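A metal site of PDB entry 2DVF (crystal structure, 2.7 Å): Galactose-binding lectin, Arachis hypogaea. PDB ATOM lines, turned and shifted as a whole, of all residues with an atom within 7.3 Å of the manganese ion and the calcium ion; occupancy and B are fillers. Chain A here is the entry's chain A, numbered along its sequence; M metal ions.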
ATOM      1  N   ALA A  82      -4.140  12.871  28.901  1.00  0.00           N
ATOM      2  CA  ALA A  82      -2.756  12.779  29.306  1.00  0.00           C
ATOM      3  C   ALA A  82      -2.586  11.411  29.953  1.00  0.00           C
ATOM      4  O   ALA A  82      -3.587  10.782  30.323  1.00  0.00           O
ATOM      5  CB  ALA A  82      -2.430  13.883  30.293  1.00  0.00           C
ATOM      6  N   ASP A  83      -1.351  10.945  30.111  1.00  0.00           N
ATOM      7  CA  ASP A  83      -0.159  11.695  29.712  1.00  0.00           C
ATOM      8  C   ASP A  83       0.558  11.142  28.478  1.00  0.00           C
ATOM      9  O   ASP A  83       1.296  11.865  27.811  1.00  0.00           O
ATOM     10  CB  ASP A  83       0.815  11.751  30.898  1.00  0.00           C
ATOM     11  CG  ASP A  83       0.756  13.070  31.626  1.00  0.00           C
ATOM     12  OD1 ASP A  83       1.497  13.997  31.218  1.00  0.00           O
ATOM     13  OD2 ASP A  83      -0.011  13.202  32.600  1.00  0.00           O
ATOM     14  N   GLY A  84       0.346   9.863  28.187  1.00  0.00           N
ATOM     15  CA  GLY A  84       0.994   9.272  27.030  1.00  0.00           C
ATOM     16  C   GLY A  84       1.477   7.848  27.194  1.00  0.00           C
ATOM     17  O   GLY A  84       1.327   7.241  28.249  1.00  0.00           O
ATOM     18  N   GLY A 103       2.246  11.499  35.575  1.00  0.00           N
ATOM     19  CA  GLY A 103       2.273  12.622  34.664  1.00  0.00           C
ATOM     20  C   GLY A 103       3.269  12.563  33.514  1.00  0.00           C
ATOM     21  O   GLY A 103       3.363  11.562  32.803  1.00  0.00           O
ATOM     22  N   GLY A 104       3.995  13.658  33.335  1.00  0.00           N
ATOM     23  CA  GLY A 104       4.971  13.746  32.264  1.00  0.00           C
ATOM     24  C   GLY A 104       6.201  12.866  32.408  1.00  0.00           C
ATOM     25  O   GLY A 104       7.115  12.958  31.586  1.00  0.00           O
ATOM     26  N   THR A 105       6.260  12.022  33.429  1.00  0.00           N
ATOM     27  CA  THR A 105       7.424  11.156  33.602  1.00  0.00           C
ATOM     28  C   THR A 105       7.206   9.865  32.817  1.00  0.00           C
ATOM     29  O   THR A 105       8.140   9.091  32.617  1.00  0.00           O
ATOM     30  CB  THR A 105       7.645  10.789  35.074  1.00  0.00           C
ATOM     31  OG1 THR A 105       6.718   9.749  35.451  1.00  0.00           O
ATOM     32  CG2 THR A 105       7.420  12.011  35.960  1.00  0.00           C
ATOM     33  N   LEU A 106       5.966   9.658  32.394  1.00  0.00           N
ATOM     34  CA  LEU A 106       5.541   8.497  31.628  1.00  0.00           C
ATOM     35  C   LEU A 106       5.811   7.177  32.325  1.00  0.00           C
ATOM     36  O   LEU A 106       5.764   6.112  31.709  1.00  0.00           O
ATOM     37  CB  LEU A 106       6.204   8.517  30.249  1.00  0.00           C
ATOM     38  CG  LEU A 106       5.994   9.802  29.453  1.00  0.00           C
ATOM     39  CD1 LEU A 106       6.548   9.627  28.040  1.00  0.00           C
ATOM     40  CD2 LEU A 106       4.511  10.169  29.401  1.00  0.00           C
ATOM     41  N   GLU A 121       8.588   7.952  22.909  1.00  0.00           N
ATOM     42  CA  GLU A 121       7.385   8.382  23.582  1.00  0.00           C
ATOM     43  C   GLU A 121       6.305   8.911  22.632  1.00  0.00           C
ATOM     44  O   GLU A 121       6.585   9.341  21.515  1.00  0.00           O
ATOM     45  CB  GLU A 121       7.711   9.433  24.639  1.00  0.00           C
ATOM     46  CG  GLU A 121       8.370  10.677  24.099  1.00  0.00           C
ATOM     47  CD  GLU A 121       8.287  11.815  25.076  1.00  0.00           C
ATOM     48  OE1 GLU A 121       8.877  11.713  26.161  1.00  0.00           O
ATOM     49  OE2 GLU A 121       7.617  12.817  24.759  1.00  0.00           O
ATOM     50  N   PHE A 122       5.074   8.837  23.120  1.00  0.00           N
ATOM     51  CA  PHE A 122       3.901   9.296  22.390  1.00  0.00           C
ATOM     52  C   PHE A 122       3.211  10.210  23.381  1.00  0.00           C
ATOM     53  O   PHE A 122       2.193   9.878  24.005  1.00  0.00           O
ATOM     54  CB  PHE A 122       3.057   8.090  21.995  1.00  0.00           C
ATOM     55  CG  PHE A 122       3.775   7.134  21.089  1.00  0.00           C
ATOM     56  CD1 PHE A 122       3.856   7.380  19.717  1.00  0.00           C
ATOM     57  CD2 PHE A 122       4.445   6.028  21.615  1.00  0.00           C
ATOM     58  CE1 PHE A 122       4.577   6.520  18.885  1.00  0.00           C
ATOM     59  CE2 PHE A 122       5.170   5.177  20.792  1.00  0.00           C
ATOM     60  CZ  PHE A 122       5.238   5.416  19.422  1.00  0.00           C
ATOM     61  N   ASP A 123       3.829  11.369  23.509  1.00  0.00           N
ATOM     62  CA  ASP A 123       3.440  12.427  24.419  1.00  0.00           C
ATOM     63  C   ASP A 123       2.184  13.197  23.982  1.00  0.00           C
ATOM     64  O   ASP A 123       2.138  13.780  22.900  1.00  0.00           O
ATOM     65  CB  ASP A 123       4.625  13.366  24.572  1.00  0.00           C
ATOM     66  CG  ASP A 123       4.677  14.041  25.910  1.00  0.00           C
ATOM     67  OD1 ASP A 123       3.596  14.425  26.406  1.00  0.00           O
ATOM     68  OD2 ASP A 123       5.787  14.201  26.458  1.00  0.00           O
ATOM     69  N   THR A 124       1.183  13.202  24.848  1.00  0.00           N
ATOM     70  CA  THR A 124      -0.080  13.869  24.559  1.00  0.00           C
ATOM     71  C   THR A 124      -0.324  15.054  25.487  1.00  0.00           C
ATOM     72  O   THR A 124      -1.426  15.611  25.507  1.00  0.00           O
ATOM     73  CB  THR A 124      -1.240  12.913  24.725  1.00  0.00           C
ATOM     74  OG1 THR A 124      -1.378  12.571  26.100  1.00  0.00           O
ATOM     75  CG2 THR A 124      -1.004  11.635  23.926  1.00  0.00           C
ATOM     76  N   TYR A 125       0.679  15.416  26.276  1.00  0.00           N
ATOM     77  CA  TYR A 125       0.552  16.548  27.178  1.00  0.00           C
ATOM     78  C   TYR A 125       1.846  17.350  27.242  1.00  0.00           C
ATOM     79  O   TYR A 125       2.898  16.815  27.591  1.00  0.00           O
ATOM     80  CB  TYR A 125       0.149  16.060  28.580  1.00  0.00           C
ATOM     81  CG  TYR A 125      -0.178  17.181  29.545  1.00  0.00           C
ATOM     82  CD1 TYR A 125       0.829  17.849  30.244  1.00  0.00           C
ATOM     83  CD2 TYR A 125      -1.493  17.594  29.737  1.00  0.00           C
ATOM     84  CE1 TYR A 125       0.540  18.902  31.112  1.00  0.00           C
ATOM     85  CE2 TYR A 125      -1.804  18.644  30.618  1.00  0.00           C
ATOM     86  CZ  TYR A 125      -0.787  19.287  31.294  1.00  0.00           C
ATOM     87  OH  TYR A 125      -1.076  20.319  32.151  1.00  0.00           O
ATOM     88  N   SER A 126       1.781  18.629  26.902  1.00  0.00           N
ATOM     89  CA  SER A 126       2.974  19.467  26.910  1.00  0.00           C
ATOM     90  C   SER A 126       3.455  19.889  28.298  1.00  0.00           C
ATOM     91  O   SER A 126       2.888  20.775  28.921  1.00  0.00           O
ATOM     92  CB  SER A 126       2.731  20.711  26.055  1.00  0.00           C
ATOM     93  OG  SER A 126       3.872  21.537  26.028  1.00  0.00           O
ATOM     94  N   ASN A 127       4.525  19.242  28.772  1.00  0.00           N
ATOM     95  CA  ASN A 127       5.127  19.532  30.070  1.00  0.00           C
ATOM     96  C   ASN A 127       6.333  20.428  29.846  1.00  0.00           C
ATOM     97  O   ASN A 127       7.382  19.961  29.422  1.00  0.00           O
ATOM     98  CB  ASN A 127       5.596  18.256  30.765  1.00  0.00           C
ATOM     99  CG  ASN A 127       4.458  17.434  31.296  1.00  0.00           C
ATOM    100  OD1 ASN A 127       3.666  16.899  30.546  1.00  0.00           O
ATOM    101  ND2 ASN A 127       4.360  17.333  32.614  1.00  0.00           N
ATOM    102  N   SER A 128       6.197  21.717  30.160  1.00  0.00           N
ATOM    103  CA  SER A 128       7.297  22.663  29.981  1.00  0.00           C
ATOM    104  C   SER A 128       8.487  22.338  30.865  1.00  0.00           C
ATOM    105  O   SER A 128       9.620  22.673  30.529  1.00  0.00           O
ATOM    106  CB  SER A 128       6.809  24.083  30.270  1.00  0.00           C
ATOM    107  OG  SER A 128       6.366  24.206  31.608  1.00  0.00           O
ATOM    108  N   TYR A 130       9.770  19.713  31.183  1.00  0.00           N
ATOM    109  CA  TYR A 130      10.544  18.685  30.490  1.00  0.00           C
ATOM    110  C   TYR A 130      10.790  19.189  29.077  1.00  0.00           C
ATOM    111  O   TYR A 130      11.225  18.444  28.203  1.00  0.00           O
ATOM    112  CB  TYR A 130       9.777  17.358  30.444  1.00  0.00           C
ATOM    113  CG  TYR A 130       9.365  16.830  31.805  1.00  0.00           C
ATOM    114  CD1 TYR A 130      10.287  16.712  32.850  1.00  0.00           C
ATOM    115  CD2 TYR A 130       8.051  16.422  32.039  1.00  0.00           C
ATOM    116  CE1 TYR A 130       9.908  16.202  34.086  1.00  0.00           C
ATOM    117  CE2 TYR A 130       7.663  15.916  33.277  1.00  0.00           C
ATOM    118  CZ  TYR A 130       8.594  15.805  34.290  1.00  0.00           C
ATOM    119  OH  TYR A 130       8.208  15.308  35.518  1.00  0.00           O
ATOM    120  N   ASN A 131      10.482  20.463  28.866  1.00  0.00           N
ATOM    121  CA  ASN A 131      10.658  21.111  27.568  1.00  0.00           C
ATOM    122  C   ASN A 131       9.832  20.468  26.465  1.00  0.00           C
ATOM    123  O   ASN A 131      10.276  20.390  25.331  1.00  0.00           O
ATOM    124  CB  ASN A 131      12.140  21.103  27.179  1.00  0.00           C
ATOM    125  CG  ASN A 131      12.966  22.000  28.059  1.00  0.00           C
ATOM    126  OD1 ASN A 131      12.797  23.225  28.061  1.00  0.00           O
ATOM    127  ND2 ASN A 131      13.878  21.404  28.825  1.00  0.00           N
ATOM    128  N   ASP A 132       8.631  20.009  26.795  1.00  0.00           N
ATOM    129  CA  ASP A 132       7.774  19.389  25.797  1.00  0.00           C
ATOM    130  C   ASP A 132       7.427  20.360  24.684  1.00  0.00           C
ATOM    131  O   ASP A 132       7.301  21.560  24.913  1.00  0.00           O
ATOM    132  CB  ASP A 132       6.454  18.880  26.422  1.00  0.00           C
ATOM    133  CG  ASP A 132       6.535  17.447  26.906  1.00  0.00           C
ATOM    134  OD1 ASP A 132       7.362  16.679  26.376  1.00  0.00           O
ATOM    135  OD2 ASP A 132       5.754  17.083  27.793  1.00  0.00           O
ATOM    136  N   PRO A 133       7.282  19.858  23.454  1.00  0.00           N
ATOM    137  CA  PRO A 133       6.941  20.731  22.337  1.00  0.00           C
ATOM    138  C   PRO A 133       5.529  21.256  22.625  1.00  0.00           C
ATOM    139  O   PRO A 133       4.818  20.716  23.467  1.00  0.00           O
ATOM    140  CB  PRO A 133       6.962  19.796  21.142  1.00  0.00           C
ATOM    141  CG  PRO A 133       7.947  18.742  21.542  1.00  0.00           C
ATOM    142  CD  PRO A 133       7.593  18.492  22.976  1.00  0.00           C
ATOM    143  N   HIS A 137       3.382  14.981  20.334  1.00  0.00           N
ATOM    144  CA  HIS A 137       4.611  14.627  19.650  1.00  0.00           C
ATOM    145  C   HIS A 137       5.116  13.206  19.892  1.00  0.00           C
ATOM    146  O   HIS A 137       4.751  12.540  20.870  1.00  0.00           O
ATOM    147  CB  HIS A 137       5.705  15.602  20.067  1.00  0.00           C
ATOM    148  CG  HIS A 137       5.902  15.660  21.547  1.00  0.00           C
ATOM    149  ND1 HIS A 137       5.035  16.329  22.380  1.00  0.00           N
ATOM    150  CD2 HIS A 137       6.845  15.105  22.352  1.00  0.00           C
ATOM    151  CE1 HIS A 137       5.425  16.175  23.638  1.00  0.00           C
ATOM    152  NE2 HIS A 137       6.527  15.437  23.641  1.00  0.00           N
ATOM    153  N   VAL A 138       5.977  12.752  18.987  1.00  0.00           N
ATOM    154  CA  VAL A 138       6.615  11.451  19.087  1.00  0.00           C
ATOM    155  C   VAL A 138       8.065  11.824  19.420  1.00  0.00           C
ATOM    156  O   VAL A 138       8.602  12.761  18.824  1.00  0.00           O
ATOM    157  CB  VAL A 138       6.578  10.674  17.743  1.00  0.00           C
ATOM    158  CG1 VAL A 138       7.298   9.353  17.873  1.00  0.00           C
ATOM    159  CG2 VAL A 138       5.143  10.433  17.322  1.00  0.00           C
ATOM    160  N   GLY A 139       8.679  11.137  20.370  1.00  0.00           N
ATOM    161  CA  GLY A 139      10.038  11.490  20.713  1.00  0.00           C
ATOM    162  C   GLY A 139      10.968  10.361  21.076  1.00  0.00           C
ATOM    163  O   GLY A 139      10.535   9.299  21.514  1.00  0.00           O
ATOM    164  N   ASP A 141      13.725   9.226  23.558  1.00  0.00           N
ATOM    165  CA  ASP A 141      14.217   9.557  24.881  1.00  0.00           C
ATOM    166  C   ASP A 141      15.452   8.753  25.259  1.00  0.00           C
ATOM    167  O   ASP A 141      15.540   7.555  24.975  1.00  0.00           O
ATOM    168  CB  ASP A 141      13.116   9.345  25.923  1.00  0.00           C
ATOM    169  CG  ASP A 141      11.894  10.221  25.687  1.00  0.00           C
ATOM    170  OD1 ASP A 141      12.045  11.311  25.082  1.00  0.00           O
ATOM    171  OD2 ASP A 141      10.795   9.831  26.107  1.00  0.00           O
ATOM    172  N   SER A 144      15.812  10.356  29.807  1.00  0.00           N
ATOM    173  CA  SER A 144      15.081  11.557  30.169  1.00  0.00           C
ATOM    174  C   SER A 144      13.825  11.769  29.349  1.00  0.00           C
ATOM    175  O   SER A 144      13.811  11.464  28.151  1.00  0.00           O
ATOM    176  CB  SER A 144      15.970  12.794  30.015  1.00  0.00           C
ATOM    177  OG  SER A 144      15.194  13.978  30.089  1.00  0.00           O
ATOM    178  N   VAL A 145      12.763  12.274  29.978  1.00  0.00           N
ATOM    179  CA  VAL A 145      11.529  12.542  29.248  1.00  0.00           C
ATOM    180  C   VAL A 145      11.678  13.888  28.552  1.00  0.00           C
ATOM    181  O   VAL A 145      10.733  14.392  27.958  1.00  0.00           O
ATOM    182  CB  VAL A 145      10.272  12.567  30.146  1.00  0.00           C
ATOM    183  CG1 VAL A 145       9.861  11.155  30.508  1.00  0.00           C
ATOM    184  CG2 VAL A 145      10.514  13.416  31.376  1.00  0.00           C
ATOM    185  N   ASP A 146      12.872  14.460  28.661  1.00  0.00           N
ATOM    186  CA  ASP A 146      13.172  15.697  27.953  1.00  0.00           C
ATOM    187  C   ASP A 146      13.803  15.090  26.707  1.00  0.00           C
ATOM    188  O   ASP A 146      15.012  14.898  26.636  1.00  0.00           O
ATOM    189  CB  ASP A 146      14.213  16.524  28.704  1.00  0.00           C
ATOM    190  CG  ASP A 146      14.530  17.839  27.987  1.00  0.00           C
ATOM    191  OD1 ASP A 146      14.648  17.848  26.744  1.00  0.00           O
ATOM    192  OD2 ASP A 146      14.683  18.876  28.670  1.00  0.00           O
ATOM    193  N   SER A 147      12.973  14.769  25.727  1.00  0.00           N
ATOM    194  CA  SER A 147      13.423  14.133  24.502  1.00  0.00           C
ATOM    195  C   SER A 147      14.669  14.744  23.840  1.00  0.00           C
ATOM    196  O   SER A 147      14.918  15.942  23.903  1.00  0.00           O
ATOM    197  CB  SER A 147      12.268  14.103  23.491  1.00  0.00           C
ATOM    198  OG  SER A 147      11.079  13.631  24.110  1.00  0.00           O
ATOM    199  N   THR A 150      12.176  15.354  18.991  1.00  0.00           N
ATOM    200  CA  THR A 150      10.728  15.143  18.955  1.00  0.00           C
ATOM    201  C   THR A 150      10.260  15.431  17.540  1.00  0.00           C
ATOM    202  O   THR A 150      11.000  16.003  16.736  1.00  0.00           O
ATOM    203  CB  THR A 150       9.981  16.078  19.944  1.00  0.00           C
ATOM    204  OG1 THR A 150      10.196  17.456  19.574  1.00  0.00           O
ATOM    205  CG2 THR A 150      10.481  15.874  21.359  1.00  0.00           C
HETATM  206 MN    MN M   1       7.984  14.798  25.470  1.00  0.00          MN
HETATM  207 CA    CA M   2       4.367  15.099  28.715  1.00  0.00          CA
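OE1 of Glu 121 lies close to OD2 of Asp 141 (2.7 Å).
The backbone carbonyl oxygen (O) of Asp 83 sits at hydrogen-bond distance from the side-chain hydroxyl (OG1) of Thr 124 (3.3 Å).
The backbone carbonyl oxygen (O) of Gly 139 sits at hydrogen-bond distance from the backbone NH (N) of Glu 121, 2.7 Å away.
The side-chain carboxylate (OD1) of Asp 83 lies within hydrogen-bond range of the backbone NH (N) of Gly 104.
The side-chain hydroxyl (OG) of Ser 147 sits at hydrogen-bond distance from the side-chain carboxylate (OD1) of Asp 141, 2.7 Å away.
Residues that only touch the manganese ion: Val 145 and Ser 147.
Merely in contact with the calcium ion: Gly 104 (3.8 Å) and Asp 83 (3.96 Å).
Within 4 Å of the calcium ion: Asp 83, Gly 104, Asp 123, Tyr 125, Asn 127 and Asp 132.
Along chain A the residues within 4 Å of the calcium ion span positions 83 to 132.
The manganese ion is bound by the side-chain carboxylate of Glu 121, the side-chain carboxylate of Asp 132, a ring nitrogen (NE2) of His 137 and the side-chain carboxylate of Asp 123.
The manganese ion has four donor atoms within binding distance.
The calcium ion is bound by O of Tyr 125 (2.5 Å), OD1 of Asp 123 (2.5 Å), OD2 of Asp 132 (2.6 Å), OD1 of Asn 127 (2.7 Å) and OD2 of Asp 123 (2.8 Å).
The calcium ion has five donor atoms within binding distance.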
